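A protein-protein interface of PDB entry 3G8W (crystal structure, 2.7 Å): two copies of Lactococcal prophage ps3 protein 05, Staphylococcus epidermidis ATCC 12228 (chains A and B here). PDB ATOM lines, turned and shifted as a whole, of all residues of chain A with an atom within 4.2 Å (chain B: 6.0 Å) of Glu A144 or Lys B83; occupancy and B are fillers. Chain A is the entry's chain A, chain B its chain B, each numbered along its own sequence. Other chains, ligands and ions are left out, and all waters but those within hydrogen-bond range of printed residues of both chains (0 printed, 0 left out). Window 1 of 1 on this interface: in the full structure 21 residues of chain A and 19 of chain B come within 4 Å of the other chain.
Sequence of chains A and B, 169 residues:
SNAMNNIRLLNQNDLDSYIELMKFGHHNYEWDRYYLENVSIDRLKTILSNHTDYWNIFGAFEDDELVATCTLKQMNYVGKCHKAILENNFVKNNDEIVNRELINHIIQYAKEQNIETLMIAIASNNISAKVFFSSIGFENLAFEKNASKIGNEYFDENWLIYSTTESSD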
ATOM      1  N   ALA A 142      -2.892  33.330   6.376  1.00  0.00           N
ATOM      2  CA  ALA A 142      -2.282  32.223   7.105  1.00  0.00           C
ATOM      3  C   ALA A 142      -0.862  32.478   7.529  1.00  0.00           C
ATOM      4  O   ALA A 142      -0.181  33.355   7.030  1.00  0.00           O
ATOM      5  CB  ALA A 142      -2.325  30.998   6.251  1.00  0.00           C
ATOM      6  N   PHE A 143      -0.395  31.655   8.436  1.00  0.00           N
ATOM      7  CA  PHE A 143       0.914  31.804   8.999  1.00  0.00           C
ATOM      8  C   PHE A 143       1.777  30.709   8.366  1.00  0.00           C
ATOM      9  O   PHE A 143       1.421  29.545   8.396  1.00  0.00           O
ATOM     10  CB  PHE A 143       0.798  31.602  10.479  1.00  0.00           C
ATOM     11  CG  PHE A 143       2.100  31.457  11.178  1.00  0.00           C
ATOM     12  CD1 PHE A 143       2.984  32.539  11.294  1.00  0.00           C
ATOM     13  CD2 PHE A 143       2.460  30.254  11.734  1.00  0.00           C
ATOM     14  CE1 PHE A 143       4.205  32.397  11.968  1.00  0.00           C
ATOM     15  CE2 PHE A 143       3.687  30.104  12.412  1.00  0.00           C
ATOM     16  CZ  PHE A 143       4.550  31.170  12.541  1.00  0.00           C
ATOM     17  N   GLU A 144       2.905  31.076   7.776  1.00  0.00           N
ATOM     18  CA  GLU A 144       3.768  30.070   7.203  1.00  0.00           C
ATOM     19  C   GLU A 144       5.060  29.939   8.005  1.00  0.00           C
ATOM     20  O   GLU A 144       5.981  30.741   7.838  1.00  0.00           O
ATOM     21  CB  GLU A 144       4.070  30.384   5.757  1.00  0.00           C
ATOM     22  CG  GLU A 144       4.207  29.127   4.968  1.00  0.00           C
ATOM     23  CD  GLU A 144       4.984  29.286   3.672  1.00  0.00           C
ATOM     24  OE1 GLU A 144       4.753  30.254   2.936  1.00  0.00           O
ATOM     25  OE2 GLU A 144       5.811  28.421   3.358  1.00  0.00           O
ATOM     26  N   LYS A 145       5.121  28.947   8.898  1.00  0.00           N
ATOM     27  CA  LYS A 145       6.383  28.616   9.568  1.00  0.00           C
ATOM     28  C   LYS A 145       7.393  28.178   8.515  1.00  0.00           C
ATOM     29  O   LYS A 145       7.016  27.526   7.545  1.00  0.00           O
ATOM     30  CB  LYS A 145       6.192  27.505  10.585  1.00  0.00           C
ATOM     31  CG  LYS A 145       7.072  27.667  11.741  1.00  0.00           C
ATOM     32  CD  LYS A 145       7.592  26.337  12.204  1.00  0.00           C
ATOM     33  CE  LYS A 145       8.268  26.451  13.580  1.00  0.00           C
ATOM     34  NZ  LYS A 145       8.461  25.102  14.268  1.00  0.00           N
ATOM     35  N   ASN A 146       8.661  28.557   8.702  1.00  0.00           N
ATOM     36  CA  ASN A 146       9.756  28.239   7.780  1.00  0.00           C
ATOM     37  C   ASN A 146       9.399  28.482   6.322  1.00  0.00           C
ATOM     38  O   ASN A 146       9.769  27.702   5.435  1.00  0.00           O
ATOM     39  CB  ASN A 146      10.249  26.803   7.952  1.00  0.00           C
ATOM     40  CG  ASN A 146      10.575  26.457   9.375  1.00  0.00           C
ATOM     41  OD1 ASN A 146      10.226  25.395   9.845  1.00  0.00           O
ATOM     42  ND2 ASN A 146      11.252  27.337  10.065  1.00  0.00           N
ATOM     43  N   ALA A 147       8.686  29.577   6.091  1.00  0.00           N
ATOM     44  CA  ALA A 147       8.361  30.057   4.757  1.00  0.00           C
ATOM     45  C   ALA A 147       9.590  30.312   3.878  1.00  0.00           C
ATOM     46  O   ALA A 147       9.511  30.170   2.662  1.00  0.00           O
ATOM     47  CB  ALA A 147       7.565  31.308   4.852  1.00  0.00           C
ATOM     48  N   ASP A 156       9.694  32.850   9.369  1.00  0.00           N
ATOM     49  CA  ASP A 156       8.258  32.689   9.310  1.00  0.00           C
ATOM     50  C   ASP A 156       7.614  33.888   8.644  1.00  0.00           C
ATOM     51  O   ASP A 156       8.072  35.003   8.793  1.00  0.00           O
ATOM     52  CB  ASP A 156       7.717  32.483  10.716  1.00  0.00           C
ATOM     53  CG  ASP A 156       8.585  31.559  11.523  1.00  0.00           C
ATOM     54  OD1 ASP A 156       9.274  30.703  10.913  1.00  0.00           O
ATOM     55  OD2 ASP A 156       8.599  31.684  12.764  1.00  0.00           O
ATOM     56  N   GLU A 157       6.564  33.642   7.876  1.00  0.00           N
ATOM     57  CA  GLU A 157       5.834  34.717   7.212  1.00  0.00           C
ATOM     58  C   GLU A 157       4.376  34.499   7.468  1.00  0.00           C
ATOM     59  O   GLU A 157       3.965  33.383   7.774  1.00  0.00           O
ATOM     60  CB  GLU A 157       6.094  34.731   5.698  1.00  0.00           C
ATOM     61  CG  GLU A 157       7.361  35.447   5.333  1.00  0.00           C
ATOM     62  CD  GLU A 157       8.084  34.891   4.095  1.00  0.00           C
ATOM     63  OE1 GLU A 157       7.463  34.214   3.245  1.00  0.00           O
ATOM     64  OE2 GLU A 157       9.286  35.173   3.942  1.00  0.00           O
ATOM     65  N   TRP A 159       0.800  35.290   5.305  1.00  0.00           N
ATOM     66  CA  TRP A 159       0.230  35.721   4.051  1.00  0.00           C
ATOM     67  C   TRP A 159      -0.939  36.589   4.369  1.00  0.00           C
ATOM     68  O   TRP A 159      -1.819  36.203   5.140  1.00  0.00           O
ATOM     69  CB  TRP A 159      -0.215  34.534   3.213  1.00  0.00           C
ATOM     70  CG  TRP A 159       0.932  33.733   2.660  1.00  0.00           C
ATOM     71  CD1 TRP A 159       1.538  32.679   3.254  1.00  0.00           C
ATOM     72  CD2 TRP A 159       1.604  33.946   1.425  1.00  0.00           C
ATOM     73  NE1 TRP A 159       2.557  32.235   2.487  1.00  0.00           N
ATOM     74  CE2 TRP A 159       2.612  32.974   1.337  1.00  0.00           C
ATOM     75  CE3 TRP A 159       1.447  34.868   0.365  1.00  0.00           C
ATOM     76  CZ2 TRP A 159       3.470  32.880   0.252  1.00  0.00           C
ATOM     77  CZ3 TRP A 159       2.314  34.767  -0.748  1.00  0.00           C
ATOM     78  CH2 TRP A 159       3.313  33.784  -0.776  1.00  0.00           C
ATOM     79  N   LYS B  73       6.578  20.379  -8.366  1.00  0.00           N
ATOM     80  CA  LYS B  73       7.042  21.706  -8.758  1.00  0.00           C
ATOM     81  C   LYS B  73       7.778  22.304  -7.579  1.00  0.00           C
ATOM     82  O   LYS B  73       7.179  22.691  -6.586  1.00  0.00           O
ATOM     83  CB  LYS B  73       5.868  22.594  -9.208  1.00  0.00           C
ATOM     84  CG  LYS B  73       6.256  23.796 -10.061  1.00  0.00           C
ATOM     85  CD  LYS B  73       6.739  25.019  -9.242  1.00  0.00           C
ATOM     86  CE  LYS B  73       7.552  26.002 -10.156  1.00  0.00           C
ATOM     87  NZ  LYS B  73       8.293  27.119  -9.443  1.00  0.00           N
ATOM     88  N   GLN B  74       9.093  22.318  -7.668  1.00  0.00           N
ATOM     89  CA  GLN B  74       9.918  22.916  -6.640  1.00  0.00           C
ATOM     90  C   GLN B  74       9.993  24.425  -6.910  1.00  0.00           C
ATOM     91  O   GLN B  74       9.929  24.855  -8.053  1.00  0.00           O
ATOM     92  CB  GLN B  74      11.288  22.264  -6.648  1.00  0.00           C
ATOM     93  CG  GLN B  74      12.129  22.607  -5.470  1.00  0.00           C
ATOM     94  CD  GLN B  74      13.539  22.094  -5.602  1.00  0.00           C
ATOM     95  OE1 GLN B  74      13.883  21.417  -6.573  1.00  0.00           O
ATOM     96  NE2 GLN B  74      14.368  22.411  -4.627  1.00  0.00           N
ATOM     97  N   MET B  75      10.092  25.236  -5.869  1.00  0.00           N
ATOM     98  CA  MET B  75       9.946  26.670  -6.059  1.00  0.00           C
ATOM     99  C   MET B  75      11.298  27.184  -6.351  1.00  0.00           C
ATOM    100  O   MET B  75      12.048  27.439  -5.416  1.00  0.00           O
ATOM    101  CB  MET B  75       9.485  27.363  -4.779  1.00  0.00           C
ATOM    102  CG  MET B  75       8.613  26.550  -3.904  1.00  0.00           C
ATOM    103  SD  MET B  75       6.881  27.325  -4.020  1.00  0.00           S
ATOM    104  CE  MET B  75       6.908  28.617  -2.547  1.00  0.00           C
ATOM    105  N   GLY B  79      15.279  32.025  -1.753  1.00  0.00           N
ATOM    106  CA  GLY B  79      14.913  31.571  -0.410  1.00  0.00           C
ATOM    107  C   GLY B  79      13.771  30.579  -0.294  1.00  0.00           C
ATOM    108  O   GLY B  79      13.228  30.381   0.792  1.00  0.00           O
ATOM    109  N   LYS B  80      13.380  29.966  -1.401  1.00  0.00           N
ATOM    110  CA  LYS B  80      12.197  29.121  -1.402  1.00  0.00           C
ATOM    111  C   LYS B  80      12.413  27.696  -1.924  1.00  0.00           C
ATOM    112  O   LYS B  80      11.459  26.905  -2.022  1.00  0.00           O
ATOM    113  CB  LYS B  80      11.050  29.846  -2.096  1.00  0.00           C
ATOM    114  CG  LYS B  80      10.719  31.084  -1.305  1.00  0.00           C
ATOM    115  CD  LYS B  80       9.349  31.635  -1.519  1.00  0.00           C
ATOM    116  CE  LYS B  80       8.847  32.372  -0.265  1.00  0.00           C
ATOM    117  NZ  LYS B  80       9.731  33.544   0.050  1.00  0.00           N
ATOM    118  N   CYS B  81      13.677  27.352  -2.173  1.00  0.00           N
ATOM    119  CA  CYS B  81      14.061  26.053  -2.728  1.00  0.00           C
ATOM    120  C   CYS B  81      13.883  24.876  -1.825  1.00  0.00           C
ATOM    121  O   CYS B  81      13.929  23.747  -2.294  1.00  0.00           O
ATOM    122  CB  CYS B  81      15.508  26.060  -3.160  1.00  0.00           C
ATOM    123  SG  CYS B  81      15.641  26.854  -4.711  1.00  0.00           S
ATOM    124  N   HIS B  82      13.684  25.116  -0.536  1.00  0.00           N
ATOM    125  CA  HIS B  82      13.452  24.002   0.359  1.00  0.00           C
ATOM    126  C   HIS B  82      12.013  23.496   0.249  1.00  0.00           C
ATOM    127  O   HIS B  82      11.654  22.543   0.901  1.00  0.00           O
ATOM    128  CB  HIS B  82      13.797  24.398   1.781  1.00  0.00           C
ATOM    129  CG  HIS B  82      12.919  25.472   2.307  1.00  0.00           C
ATOM    130  ND1 HIS B  82      12.884  26.730   1.750  1.00  0.00           N
ATOM    131  CD2 HIS B  82      11.991  25.468   3.290  1.00  0.00           C
ATOM    132  CE1 HIS B  82      11.998  27.467   2.391  1.00  0.00           C
ATOM    133  NE2 HIS B  82      11.439  26.725   3.328  1.00  0.00           N
ATOM    134  N   LYS B  83      11.190  24.120  -0.585  1.00  0.00           N
ATOM    135  CA  LYS B  83       9.747  23.784  -0.644  1.00  0.00           C
ATOM    136  C   LYS B  83       9.282  23.366  -2.015  1.00  0.00           C
ATOM    137  O   LYS B  83       9.897  23.714  -3.025  1.00  0.00           O
ATOM    138  CB  LYS B  83       8.900  24.985  -0.268  1.00  0.00           C
ATOM    139  CG  LYS B  83       8.908  25.340   1.152  1.00  0.00           C
ATOM    140  CD  LYS B  83       8.941  26.819   1.281  1.00  0.00           C
ATOM    141  CE  LYS B  83       7.697  27.497   0.728  1.00  0.00           C
ATOM    142  NZ  LYS B  83       7.637  28.973   1.055  1.00  0.00           N
ATOM    143  N   ALA B  84       8.166  22.657  -2.066  1.00  0.00           N
ATOM    144  CA  ALA B  84       7.666  22.208  -3.358  1.00  0.00           C
ATOM    145  C   ALA B  84       6.199  21.912  -3.288  1.00  0.00           C
ATOM    146  O   ALA B  84       5.696  21.594  -2.228  1.00  0.00           O
ATOM    147  CB  ALA B  84       8.455  20.959  -3.852  1.00  0.00           C
ATOM    148  N   ILE B  85       5.537  22.003  -4.430  1.00  0.00           N
ATOM    149  CA  ILE B  85       4.111  21.792  -4.524  1.00  0.00           C
ATOM    150  C   ILE B  85       3.899  20.536  -5.318  1.00  0.00           C
ATOM    151  O   ILE B  85       4.586  20.316  -6.322  1.00  0.00           O
ATOM    152  CB  ILE B  85       3.440  22.908  -5.352  1.00  0.00           C
ATOM    153  CG1 ILE B  85       3.779  24.305  -4.818  1.00  0.00           C
ATOM    154  CG2 ILE B  85       1.960  22.746  -5.327  1.00  0.00           C
ATOM    155  CD1 ILE B  85       3.394  24.541  -3.374  1.00  0.00           C
ATOM    156  N   ILE B 115      14.535  18.928  -0.618  1.00  0.00           N
ATOM    157  CA  ILE B 115      13.274  19.603  -0.413  1.00  0.00           C
ATOM    158  C   ILE B 115      12.745  19.260   0.981  1.00  0.00           C
ATOM    159  O   ILE B 115      12.497  18.107   1.297  1.00  0.00           O
ATOM    160  CB  ILE B 115      12.270  19.259  -1.543  1.00  0.00           C
ATOM    161  CG1 ILE B 115      12.807  19.816  -2.883  1.00  0.00           C
ATOM    162  CG2 ILE B 115      10.844  19.759  -1.197  1.00  0.00           C
ATOM    163  CD1 ILE B 115      12.316  19.102  -4.172  1.00  0.00           C
ATOM    164  N   GLU B 116      12.612  20.277   1.816  1.00  0.00           N
ATOM    165  CA  GLU B 116      12.217  20.096   3.198  1.00  0.00           C
ATOM    166  C   GLU B 116      10.735  19.942   3.427  1.00  0.00           C
ATOM    167  O   GLU B 116      10.316  19.248   4.354  1.00  0.00           O
ATOM    168  CB  GLU B 116      12.723  21.258   4.025  1.00  0.00           C
ATOM    169  CG  GLU B 116      13.845  20.888   4.916  1.00  0.00           C
ATOM    170  CD  GLU B 116      14.900  21.934   4.936  1.00  0.00           C
ATOM    171  OE1 GLU B 116      14.660  23.011   5.516  1.00  0.00           O
ATOM    172  OE2 GLU B 116      15.975  21.683   4.358  1.00  0.00           O
ATOM    173  N   THR B 117       9.920  20.617   2.625  1.00  0.00           N
ATOM    174  CA  THR B 117       8.506  20.506   2.844  1.00  0.00           C
ATOM    175  C   THR B 117       7.689  20.400   1.544  1.00  0.00           C
ATOM    176  O   THR B 117       8.042  21.001   0.526  1.00  0.00           O
ATOM    177  CB  THR B 117       7.981  21.612   3.816  1.00  0.00           C
ATOM    178  OG1 THR B 117       7.583  22.777   3.101  1.00  0.00           O
ATOM    179  CG2 THR B 117       9.002  21.979   4.910  1.00  0.00           C
ATOM    180  N   LEU B 118       6.610  19.615   1.589  1.00  0.00           N
ATOM    181  CA  LEU B 118       5.702  19.466   0.455  1.00  0.00           C
ATOM    182  C   LEU B 118       4.347  20.054   0.787  1.00  0.00           C
ATOM    183  O   LEU B 118       3.847  19.874   1.910  1.00  0.00           O
ATOM    184  CB  LEU B 118       5.528  18.004   0.066  1.00  0.00           C
ATOM    185  CG  LEU B 118       6.798  17.299  -0.420  1.00  0.00           C
ATOM    186  CD1 LEU B 118       6.529  15.822  -0.721  1.00  0.00           C
ATOM    187  CD2 LEU B 118       7.414  17.983  -1.625  1.00  0.00           C
ATOM    188  N   MET B 119       3.775  20.763  -0.188  1.00  0.00           N
ATOM    189  CA  MET B 119       2.428  21.269  -0.100  1.00  0.00           C
ATOM    190  C   MET B 119       1.554  20.830  -1.275  1.00  0.00           C
ATOM    191  O   MET B 119       2.017  20.652  -2.405  1.00  0.00           O
ATOM    192  CB  MET B 119       2.431  22.788  -0.024  1.00  0.00           C
ATOM    193  CG  MET B 119       2.678  23.374   1.342  1.00  0.00           C
ATOM    194  SD  MET B 119       3.582  25.080   1.098  1.00  0.00           S
ATOM    195  CE  MET B 119       2.149  26.261   0.598  1.00  0.00           C
ATOM    196  N   LEU B 141      -2.621  23.166   6.703  1.00  0.00           N
ATOM    197  CA  LEU B 141      -1.818  24.390   6.780  1.00  0.00           C
ATOM    198  C   LEU B 141      -2.740  25.601   6.760  1.00  0.00           C
ATOM    199  O   LEU B 141      -2.716  26.405   7.653  1.00  0.00           O
ATOM    200  CB  LEU B 141      -0.863  24.469   5.593  1.00  0.00           C
ATOM    201  CG  LEU B 141       0.083  25.676   5.528  1.00  0.00           C
ATOM    202  CD1 LEU B 141       1.174  25.642   6.616  1.00  0.00           C
ATOM    203  CD2 LEU B 141       0.714  25.758   4.166  1.00  0.00           C
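Among the printed residues, pairs that only touch across the chains: Ala A147 with Lys B80 and Ala A147 with His B82.
N of Glu A144 sits at hydrogen-bond distance from O of Glu A157, at 2.5 Å. O of His B82 lies within hydrogen-bond range of N of Thr B117 (3.1 Å). The indole nitrogen (NE1) of Trp A159 is in hydrogen-bond range of the side-chain carboxylate (OE1) of Glu A144. OD1 of Asp A156 sits at hydrogen-bond distance from N of Asn A146, at 3.1 Å. The backbone NH of Glu B116 lies within hydrogen-bond range of the backbone carbonyl oxygen of His B82. N of Met B75 lies within hydrogen-bond range of O of Lys B83.
Hydrophobic or aromatic side chains of chain B that line the printed part of chain A: His B82. Along chain B the printed residues that touch a printed residue of chain A span positions 80 to 83. Printed residues of chain A that touch a printed residue of chain B: Glu A144, Asn A146, Ala A147 and Glu A157. Among the printed residues, 6 pairs touch across the chains. Among the printed residues, Asp or Glu carboxylates within 4 Å of a Lys or Arg side-chain nitrogen of the other chain: Glu A144 with Lys B83 and Glu A157 with Lys B80.
Printed residues of chain B within 4 Å of Asn A146: His B82 (2.9 Å). Printed residues of chain B within 4 Å of Ala A147: Lys B80 (3.7 Å), His B82 (3.7 Å) and Lys B83 (2.7 Å). Of the printed residues of chain B, Glu A157 touches Lys B80. Of the printed residues of chain A, Lys B80 touches Ala A147 (3.7 Å) and Glu A157 (3.98 Å). Of the printed residues of chain A, His B82 touches Asn A146 (2.9 Å) and Ala A147 (3.7 Å). The nearest residue of chain B that does not touch Glu A144 is Met B119 (4.6 Å). The nearest printed residue of chain A that does not touch Lys B83 is Asn A146 (4.3 Å).
No position is printed for both chains.
OE2 of Glu A144 is in salt-bridge range of NZ of Lys B83. The side-chain amino group (NZ) of Lys B80 lies within salt-bridge range of the side-chain carboxylate (OE1) of Glu A157 (3.98 Å). The backbone carbonyl oxygen of Ala A147 lies within hydrogen-bond range of the side-chain amino group of Lys B83. O of Asn A146 is in hydrogen-bond range of NE2 of His B82, 2.9 Å away.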
